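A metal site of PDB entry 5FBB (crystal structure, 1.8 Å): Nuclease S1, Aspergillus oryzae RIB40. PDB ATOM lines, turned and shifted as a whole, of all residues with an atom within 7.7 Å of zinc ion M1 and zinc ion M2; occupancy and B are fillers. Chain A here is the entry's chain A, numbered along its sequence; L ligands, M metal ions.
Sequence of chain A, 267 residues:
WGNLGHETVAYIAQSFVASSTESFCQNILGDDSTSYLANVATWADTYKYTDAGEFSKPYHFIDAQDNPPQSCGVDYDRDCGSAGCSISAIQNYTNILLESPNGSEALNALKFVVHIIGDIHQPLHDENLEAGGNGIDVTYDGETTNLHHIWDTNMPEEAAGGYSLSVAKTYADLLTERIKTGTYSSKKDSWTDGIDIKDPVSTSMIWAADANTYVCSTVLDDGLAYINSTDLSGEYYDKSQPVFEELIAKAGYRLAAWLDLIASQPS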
ATOM      1  N   TRP A   1      -1.122 -17.441 -14.926  1.00  0.00           N
ATOM      2  CA  TRP A   1      -2.407 -17.834 -14.338  1.00  0.00           C
ATOM      3  C   TRP A   1      -3.466 -17.690 -15.380  1.00  0.00           C
ATOM      4  O   TRP A   1      -3.303 -16.936 -16.357  1.00  0.00           O
ATOM      5  CB  TRP A   1      -2.793 -16.904 -13.130  1.00  0.00           C
ATOM      6  CG  TRP A   1      -1.688 -16.769 -12.035  1.00  0.00           C
ATOM      7  CD1 TRP A   1      -0.808 -15.729 -11.900  1.00  0.00           C
ATOM      8  CD2 TRP A   1      -1.344 -17.714 -11.025  1.00  0.00           C
ATOM      9  NE1 TRP A   1       0.029 -15.963 -10.867  1.00  0.00           N
ATOM     10  CE2 TRP A   1      -0.273 -17.189 -10.313  1.00  0.00           C
ATOM     11  CE3 TRP A   1      -1.818 -18.992 -10.684  1.00  0.00           C
ATOM     12  CZ2 TRP A   1       0.326 -17.843  -9.250  1.00  0.00           C
ATOM     13  CZ3 TRP A   1      -1.211 -19.679  -9.647  1.00  0.00           C
ATOM     14  CH2 TRP A   1      -0.163 -19.097  -8.934  1.00  0.00           C
ATOM     15  N   GLY A   2      -4.601 -18.351 -15.134  1.00  0.00           N
ATOM     16  CA  GLY A   2      -5.793 -18.119 -15.894  1.00  0.00           C
ATOM     17  C   GLY A   2      -6.515 -16.914 -15.344  1.00  0.00           C
ATOM     18  O   GLY A   2      -5.978 -16.157 -14.484  1.00  0.00           O
ATOM     19  N   ASN A   3      -7.771 -16.728 -15.737  1.00  0.00           N
ATOM     20  CA  ASN A   3      -8.449 -15.448 -15.480  1.00  0.00           C
ATOM     21  C   ASN A   3      -8.653 -15.161 -14.010  1.00  0.00           C
ATOM     22  O   ASN A   3      -8.411 -14.030 -13.578  1.00  0.00           O
ATOM     23  CB  ASN A   3      -9.805 -15.338 -16.209  1.00  0.00           C
ATOM     24  CG  ASN A   3      -9.636 -15.295 -17.711  1.00  0.00           C
ATOM     25  OD1 ASN A   3      -8.495 -15.275 -18.256  1.00  0.00           O
ATOM     26  ND2 ASN A   3     -10.744 -15.197 -18.411  1.00  0.00           N
ATOM     27  N   GLY A   5      -6.954 -16.155 -11.458  1.00  0.00           N
ATOM     28  CA  GLY A   5      -5.670 -15.833 -10.866  1.00  0.00           C
ATOM     29  C   GLY A   5      -5.285 -14.382 -11.080  1.00  0.00           C
ATOM     30  O   GLY A   5      -4.934 -13.669 -10.122  1.00  0.00           O
ATOM     31  N   HIS A   6      -5.399 -13.914 -12.321  1.00  0.00           N
ATOM     32  CA  HIS A   6      -5.108 -12.514 -12.673  1.00  0.00           C
ATOM     33  C   HIS A   6      -6.012 -11.506 -12.056  1.00  0.00           C
ATOM     34  O   HIS A   6      -5.538 -10.451 -11.586  1.00  0.00           O
ATOM     35  CB  HIS A   6      -5.073 -12.322 -14.172  1.00  0.00           C
ATOM     36  CG  HIS A   6      -3.861 -12.936 -14.776  1.00  0.00           C
ATOM     37  ND1 HIS A   6      -2.598 -12.427 -14.527  1.00  0.00           N
ATOM     38  CD2 HIS A   6      -3.679 -14.083 -15.449  1.00  0.00           C
ATOM     39  CE1 HIS A   6      -1.704 -13.188 -15.125  1.00  0.00           C
ATOM     40  NE2 HIS A   6      -2.329 -14.231 -15.644  1.00  0.00           N
ATOM     41  N   ALA A  41      -7.120  -7.090 -16.144  1.00  0.00           N
ATOM     42  CA  ALA A  41      -6.052  -8.003 -15.703  1.00  0.00           C
ATOM     43  C   ALA A  41      -5.850  -9.170 -16.628  1.00  0.00           C
ATOM     44  O   ALA A  41      -4.788  -9.859 -16.542  1.00  0.00           O
ATOM     45  CB  ALA A  41      -6.279  -8.504 -14.302  1.00  0.00           C
ATOM     46  N   THR A  42      -6.845  -9.465 -17.458  1.00  0.00           N
ATOM     47  CA  THR A  42      -6.773 -10.588 -18.396  1.00  0.00           C
ATOM     48  C   THR A  42      -6.514 -10.173 -19.862  1.00  0.00           C
ATOM     49  O   THR A  42      -6.257 -11.042 -20.714  1.00  0.00           O
ATOM     50  CB  THR A  42      -8.103 -11.387 -18.406  1.00  0.00           C
ATOM     51  OG1 THR A  42      -9.154 -10.555 -18.898  1.00  0.00           O
ATOM     52  CG2 THR A  42      -8.455 -11.814 -17.032  1.00  0.00           C
ATOM     53  N   ALA A  44      -4.025  -8.881 -21.609  1.00  0.00           N
ATOM     54  CA  ALA A  44      -2.826  -9.355 -22.268  1.00  0.00           C
ATOM     55  C   ALA A  44      -2.961 -10.770 -22.785  1.00  0.00           C
ATOM     56  O   ALA A  44      -2.317 -11.117 -23.779  1.00  0.00           O
ATOM     57  CB  ALA A  44      -1.602  -9.233 -21.339  1.00  0.00           C
ATOM     58  N   ASP A  45      -3.736 -11.615 -22.098  1.00  0.00           N
ATOM     59  CA  ASP A  45      -4.000 -12.987 -22.532  1.00  0.00           C
ATOM     60  C   ASP A  45      -4.830 -13.059 -23.792  1.00  0.00           C
ATOM     61  O   ASP A  45      -4.613 -13.954 -24.595  1.00  0.00           O
ATOM     62  CB  ASP A  45      -4.575 -13.896 -21.463  1.00  0.00           C
ATOM     63  CG  ASP A  45      -3.468 -14.521 -20.525  1.00  0.00           C
ATOM     64  OD1 ASP A  45      -2.241 -14.408 -20.841  1.00  0.00           O
ATOM     65  OD2 ASP A  45      -3.875 -15.127 -19.445  1.00  0.00           O
ATOM     66  N   THR A  46      -5.756 -12.154 -23.996  1.00  0.00           N
ATOM     67  CA  THR A  46      -6.438 -12.044 -25.320  1.00  0.00           C
ATOM     68  C   THR A  46      -5.494 -11.556 -26.388  1.00  0.00           C
ATOM     69  O   THR A  46      -5.421 -12.119 -27.478  1.00  0.00           O
ATOM     70  CB  THR A  46      -7.619 -11.079 -25.230  1.00  0.00           C
ATOM     71  OG1 THR A  46      -8.612 -11.672 -24.413  1.00  0.00           O
ATOM     72  CG2 THR A  46      -8.217 -10.730 -26.621  1.00  0.00           C
ATOM     73  N   LYS A  48      -2.315 -11.575 -26.880  1.00  0.00           N
ATOM     74  CA  LYS A  48      -1.263 -12.410 -27.384  1.00  0.00           C
ATOM     75  C   LYS A  48      -1.737 -13.418 -28.448  1.00  0.00           C
ATOM     76  O   LYS A  48      -0.875 -14.014 -29.150  1.00  0.00           O
ATOM     77  CB  LYS A  48      -0.529 -13.141 -26.263  1.00  0.00           C
ATOM     78  CG  LYS A  48      -1.271 -14.302 -25.692  1.00  0.00           C
ATOM     79  CD  LYS A  48      -0.615 -14.816 -24.450  1.00  0.00           C
ATOM     80  CE  LYS A  48      -1.217 -16.088 -23.923  1.00  0.00           C
ATOM     81  NZ  LYS A  48      -0.488 -16.488 -22.697  1.00  0.00           N
ATOM     82  N   SER A  56       3.799 -10.103 -28.214  1.00  0.00           N
ATOM     83  CA  SER A  56       3.779 -10.084 -26.776  1.00  0.00           C
ATOM     84  C   SER A  56       3.638 -11.457 -26.110  1.00  0.00           C
ATOM     85  O   SER A  56       3.712 -11.560 -24.893  1.00  0.00           O
ATOM     86  CB  SER A  56       2.688  -9.118 -26.304  1.00  0.00           C
ATOM     87  OG  SER A  56       1.386  -9.671 -26.535  1.00  0.00           O
ATOM     88  N   LYS A  57       3.525 -12.513 -26.899  1.00  0.00           N
ATOM     89  CA  LYS A  57       3.413 -13.864 -26.326  1.00  0.00           C
ATOM     90  C   LYS A  57       4.554 -14.226 -25.381  1.00  0.00           C
ATOM     91  O   LYS A  57       4.311 -14.770 -24.296  1.00  0.00           O
ATOM     92  CB  LYS A  57       3.350 -14.944 -27.408  1.00  0.00           C
ATOM     93  CG  LYS A  57       1.995 -15.148 -28.046  1.00  0.00           C
ATOM     94  CD  LYS A  57       2.025 -16.300 -29.044  1.00  0.00           C
ATOM     95  CE  LYS A  57       2.266 -17.657 -28.347  1.00  0.00           C
ATOM     96  NZ  LYS A  57       1.200 -18.083 -27.324  1.00  0.00           N
ATOM     97  N   TYR A  59       6.190 -12.350 -23.477  1.00  0.00           N
ATOM     98  CA  TYR A  59       6.239 -11.453 -22.331  1.00  0.00           C
ATOM     99  C   TYR A  59       5.545 -12.044 -21.081  1.00  0.00           C
ATOM    100  O   TYR A  59       5.622 -11.456 -20.045  1.00  0.00           O
ATOM    101  CB  TYR A  59       5.639 -10.142 -22.647  1.00  0.00           C
ATOM    102  CG  TYR A  59       6.279  -9.343 -23.759  1.00  0.00           C
ATOM    103  CD1 TYR A  59       7.437  -9.732 -24.414  1.00  0.00           C
ATOM    104  CD2 TYR A  59       5.669  -8.167 -24.161  1.00  0.00           C
ATOM    105  CE1 TYR A  59       7.937  -8.971 -25.483  1.00  0.00           C
ATOM    106  CE2 TYR A  59       6.172  -7.437 -25.208  1.00  0.00           C
ATOM    107  CZ  TYR A  59       7.346  -7.815 -25.823  1.00  0.00           C
ATOM    108  OH  TYR A  59       7.855  -7.049 -26.872  1.00  0.00           O
ATOM    109  N   HIS A  60       4.919 -13.215 -21.202  1.00  0.00           N
ATOM    110  CA  HIS A  60       4.215 -13.872 -20.085  1.00  0.00           C
ATOM    111  C   HIS A  60       5.095 -14.725 -19.193  1.00  0.00           C
ATOM    112  O   HIS A  60       4.627 -15.218 -18.182  1.00  0.00           O
ATOM    113  CB  HIS A  60       2.974 -14.642 -20.584  1.00  0.00           C
ATOM    114  CG  HIS A  60       1.974 -13.751 -21.267  1.00  0.00           C
ATOM    115  ND1 HIS A  60       0.724 -13.463 -20.742  1.00  0.00           N
ATOM    116  CD2 HIS A  60       2.096 -12.990 -22.383  1.00  0.00           C
ATOM    117  CE1 HIS A  60       0.122 -12.588 -21.507  1.00  0.00           C
ATOM    118  NE2 HIS A  60       0.924 -12.269 -22.502  1.00  0.00           N
ATOM    119  N   PHE A  61       6.332 -14.970 -19.634  1.00  0.00           N
ATOM    120  CA  PHE A  61       7.153 -15.919 -18.941  1.00  0.00           C
ATOM    121  C   PHE A  61       8.633 -15.654 -19.148  1.00  0.00           C
ATOM    122  O   PHE A  61       9.047 -14.834 -19.928  1.00  0.00           O
ATOM    123  CB  PHE A  61       6.768 -17.379 -19.327  1.00  0.00           C
ATOM    124  CG  PHE A  61       6.879 -17.624 -20.789  1.00  0.00           C
ATOM    125  CD1 PHE A  61       8.104 -17.955 -21.377  1.00  0.00           C
ATOM    126  CD2 PHE A  61       5.762 -17.529 -21.605  1.00  0.00           C
ATOM    127  CE1 PHE A  61       8.196 -18.143 -22.761  1.00  0.00           C
ATOM    128  CE2 PHE A  61       5.867 -17.654 -22.981  1.00  0.00           C
ATOM    129  CZ  PHE A  61       7.069 -17.964 -23.560  1.00  0.00           C
ATOM    130  N   HIS A 115      -0.957  -7.540 -15.528  1.00  0.00           N
ATOM    131  CA  HIS A 115      -0.979  -8.977 -15.891  1.00  0.00           C
ATOM    132  C   HIS A 115       0.326  -9.704 -15.637  1.00  0.00           C
ATOM    133  O   HIS A 115       0.359 -10.752 -14.964  1.00  0.00           O
ATOM    134  CB  HIS A 115      -1.402  -9.120 -17.342  1.00  0.00           C
ATOM    135  CG  HIS A 115      -1.527 -10.528 -17.785  1.00  0.00           C
ATOM    136  ND1 HIS A 115      -2.721 -11.196 -17.772  1.00  0.00           N
ATOM    137  CD2 HIS A 115      -0.603 -11.408 -18.244  1.00  0.00           C
ATOM    138  CE1 HIS A 115      -2.552 -12.431 -18.183  1.00  0.00           C
ATOM    139  NE2 HIS A 115      -1.283 -12.580 -18.508  1.00  0.00           N
ATOM    140  N   ILE A 116       1.402  -9.082 -16.078  1.00  0.00           N
ATOM    141  CA  ILE A 116       2.714  -9.744 -16.083  1.00  0.00           C
ATOM    142  C   ILE A 116       3.244  -9.874 -14.675  1.00  0.00           C
ATOM    143  O   ILE A 116       3.850 -10.910 -14.338  1.00  0.00           O
ATOM    144  CB  ILE A 116       3.694  -9.074 -17.044  1.00  0.00           C
ATOM    145  CG1 ILE A 116       3.163  -9.169 -18.472  1.00  0.00           C
ATOM    146  CG2 ILE A 116       5.076  -9.710 -16.865  1.00  0.00           C
ATOM    147  CD1 ILE A 116       3.995  -8.414 -19.494  1.00  0.00           C
ATOM    148  N   GLY A 118       1.478 -10.592 -12.258  1.00  0.00           N
ATOM    149  CA  GLY A 118       0.794 -11.820 -11.827  1.00  0.00           C
ATOM    150  C   GLY A 118       1.555 -13.031 -12.387  1.00  0.00           C
ATOM    151  O   GLY A 118       1.817 -14.015 -11.646  1.00  0.00           O
ATOM    152  N   ASP A 119       1.787 -13.059 -13.667  1.00  0.00           N
ATOM    153  CA  ASP A 119       2.425 -14.224 -14.326  1.00  0.00           C
ATOM    154  C   ASP A 119       3.796 -14.589 -13.770  1.00  0.00           C
ATOM    155  O   ASP A 119       4.088 -15.776 -13.622  1.00  0.00           O
ATOM    156  CB  ASP A 119       2.563 -14.088 -15.844  1.00  0.00           C
ATOM    157  CG  ASP A 119       1.322 -14.488 -16.593  1.00  0.00           C
ATOM    158  OD1 ASP A 119       0.429 -15.196 -16.002  1.00  0.00           O
ATOM    159  OD2 ASP A 119       1.197 -14.081 -17.788  1.00  0.00           O
ATOM    160  N   ILE A 120       4.554 -13.588 -13.350  1.00  0.00           N
ATOM    161  CA  ILE A 120       5.870 -13.777 -12.767  1.00  0.00           C
ATOM    162  C   ILE A 120       5.759 -14.663 -11.524  1.00  0.00           C
ATOM    163  O   ILE A 120       6.689 -15.418 -11.241  1.00  0.00           O
ATOM    164  CB  ILE A 120       6.590 -12.453 -12.540  1.00  0.00           C
ATOM    165  CG1 ILE A 120       7.029 -11.874 -13.870  1.00  0.00           C
ATOM    166  CG2 ILE A 120       7.810 -12.634 -11.651  1.00  0.00           C
ATOM    167  CD1 ILE A 120       7.514 -10.387 -13.793  1.00  0.00           C
ATOM    168  N   GLN A 122       3.551 -17.166 -10.998  1.00  0.00           N
ATOM    169  CA  GLN A 122       3.171 -18.529 -11.297  1.00  0.00           C
ATOM    170  C   GLN A 122       4.492 -19.253 -11.549  1.00  0.00           C
ATOM    171  O   GLN A 122       5.147 -18.964 -12.519  1.00  0.00           O
ATOM    172  CB  GLN A 122       2.217 -18.565 -12.480  1.00  0.00           C
ATOM    173  CG  GLN A 122       1.275 -19.762 -12.518  1.00  0.00           C
ATOM    174  CD  GLN A 122       1.913 -21.101 -12.908  1.00  0.00           C
ATOM    175  OE1 GLN A 122       2.851 -21.576 -12.278  1.00  0.00           O
ATOM    176  NE2 GLN A 122       1.345 -21.741 -13.960  1.00  0.00           N
ATOM    177  N   HIS A 125       5.630 -20.259 -15.038  1.00  0.00           N
ATOM    178  CA  HIS A 125       5.977 -19.166 -15.921  1.00  0.00           C
ATOM    179  C   HIS A 125       7.447 -18.722 -15.747  1.00  0.00           C
ATOM    180  O   HIS A 125       7.902 -17.745 -16.385  1.00  0.00           O
ATOM    181  CB  HIS A 125       5.010 -17.970 -15.651  1.00  0.00           C
ATOM    182  CG  HIS A 125       3.675 -18.135 -16.318  1.00  0.00           C
ATOM    183  ND1 HIS A 125       3.245 -17.317 -17.329  1.00  0.00           N
ATOM    184  CD2 HIS A 125       2.696 -19.061 -16.132  1.00  0.00           C
ATOM    185  CE1 HIS A 125       2.064 -17.711 -17.751  1.00  0.00           C
ATOM    186  NE2 HIS A 125       1.700 -18.781 -17.041  1.00  0.00           N
ATOM    187  N   HIS A 148       0.965 -27.459 -16.342  1.00  0.00           N
ATOM    188  CA  HIS A 148       0.832 -25.996 -16.419  1.00  0.00           C
ATOM    189  C   HIS A 148      -0.594 -25.537 -16.124  1.00  0.00           C
ATOM    190  O   HIS A 148      -0.850 -24.610 -15.362  1.00  0.00           O
ATOM    191  CB  HIS A 148       1.267 -25.499 -17.780  1.00  0.00           C
ATOM    192  CG  HIS A 148       1.423 -24.019 -17.822  1.00  0.00           C
ATOM    193  ND1 HIS A 148       2.641 -23.397 -17.645  1.00  0.00           N
ATOM    194  CD2 HIS A 148       0.505 -23.040 -17.905  1.00  0.00           C
ATOM    195  CE1 HIS A 148       2.462 -22.094 -17.681  1.00  0.00           C
ATOM    196  NE2 HIS A 148       1.183 -21.858 -17.842  1.00  0.00           N
ATOM    197  N   ASP A 152      -2.185 -22.975 -13.484  1.00  0.00           N
ATOM    198  CA  ASP A 152      -2.883 -21.751 -13.936  1.00  0.00           C
ATOM    199  C   ASP A 152      -4.337 -21.620 -13.469  1.00  0.00           C
ATOM    200  O   ASP A 152      -4.811 -20.501 -13.170  1.00  0.00           O
ATOM    201  CB  ASP A 152      -2.905 -21.647 -15.473  1.00  0.00           C
ATOM    202  CG  ASP A 152      -1.636 -20.919 -16.082  1.00  0.00           C
ATOM    203  OD1 ASP A 152      -0.771 -20.345 -15.351  1.00  0.00           O
ATOM    204  OD2 ASP A 152      -1.602 -20.878 -17.322  1.00  0.00           O
HETATM  205  P1  LIG L   1      -1.203 -17.214 -18.932  1.00  0.00           P
HETATM  206  O1  LIG L   1      -1.078 -18.278 -17.855  1.00  0.00           O
HETATM  207  O2  LIG L   1      -0.186 -17.103 -20.077  1.00  0.00           O
HETATM  208  O3  LIG L   1      -1.178 -15.756 -18.406  1.00  0.00           O
HETATM  209  O4  LIG L   1      -2.593 -17.558 -19.579  1.00  0.00           O
HETATM  210 ZN    ZN M   1      -0.320 -14.289 -19.150  1.00  0.00          ZN
HETATM  211 ZN    ZN M   2      -1.436 -15.953 -16.374  1.00  0.00          ZN
HETATM  212 ZN    ZN M   3       0.146 -19.968 -17.864  1.00  0.00          ZN
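The nearest printed residue that does not touch zinc ion M1 is His 6 (4.04 Å).
The backbone carbonyl oxygen of His 60 sits at hydrogen-bond distance from a ring nitrogen (ND1) of His 125, at 2.7 Å.
O of His 115 lies close to ND1 of His 6.
The backbone carbonyl oxygen (O) of Ala 41 is in hydrogen-bond range of a ring nitrogen (ND1) of His 115, 2.8 Å away.
OD1 of Asp 152 lies close to N of Trp 1 (3.0 Å).
NZ of Lys 48 sits close to OD1 of Asp 45 (3.3 Å).
NE1 of Trp 1 sits at hydrogen-bond distance from O of Gly 118, 2.8 Å away.
Four residues have an atom within 4 Å of zinc ion M2: Trp 1, His 6, His 115 and Asp 119.
Along chain A the residues within 4 Å of zinc ion M2 span positions 1 to 119.
The nearest printed residue that does not touch zinc ion M2 is Asp 45 (4.01 Å).
OD1 of Asp 119 binds zinc ion M2, 2.0 Å away.
O3 of the ligand is bound to zinc ion M2 (2.1 Å).
Zinc ion M2 is bound by a ring nitrogen (NE2) of His 6, 2.1 Å away.
N of Trp 1 is bound to zinc ion M2, 2.1 Å away.
O of Trp 1 binds zinc ion M2.
Slightly farther from zinc ion M2 lies O1 of the ligand (2.8 Å).
O3 of the ligand binds zinc ion M1, 1.9 Å away.
OD2 of Asp 119 binds zinc ion M1 (2.0 Å).
Zinc ion M1 is bound by NE2 of His 115 (2.1 Å).
A ring nitrogen (ND1) of His 60 is bound to zinc ion M1 (2.1 Å).
OD1 of Asp 45 is bound to zinc ion M1 (2.6 Å).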
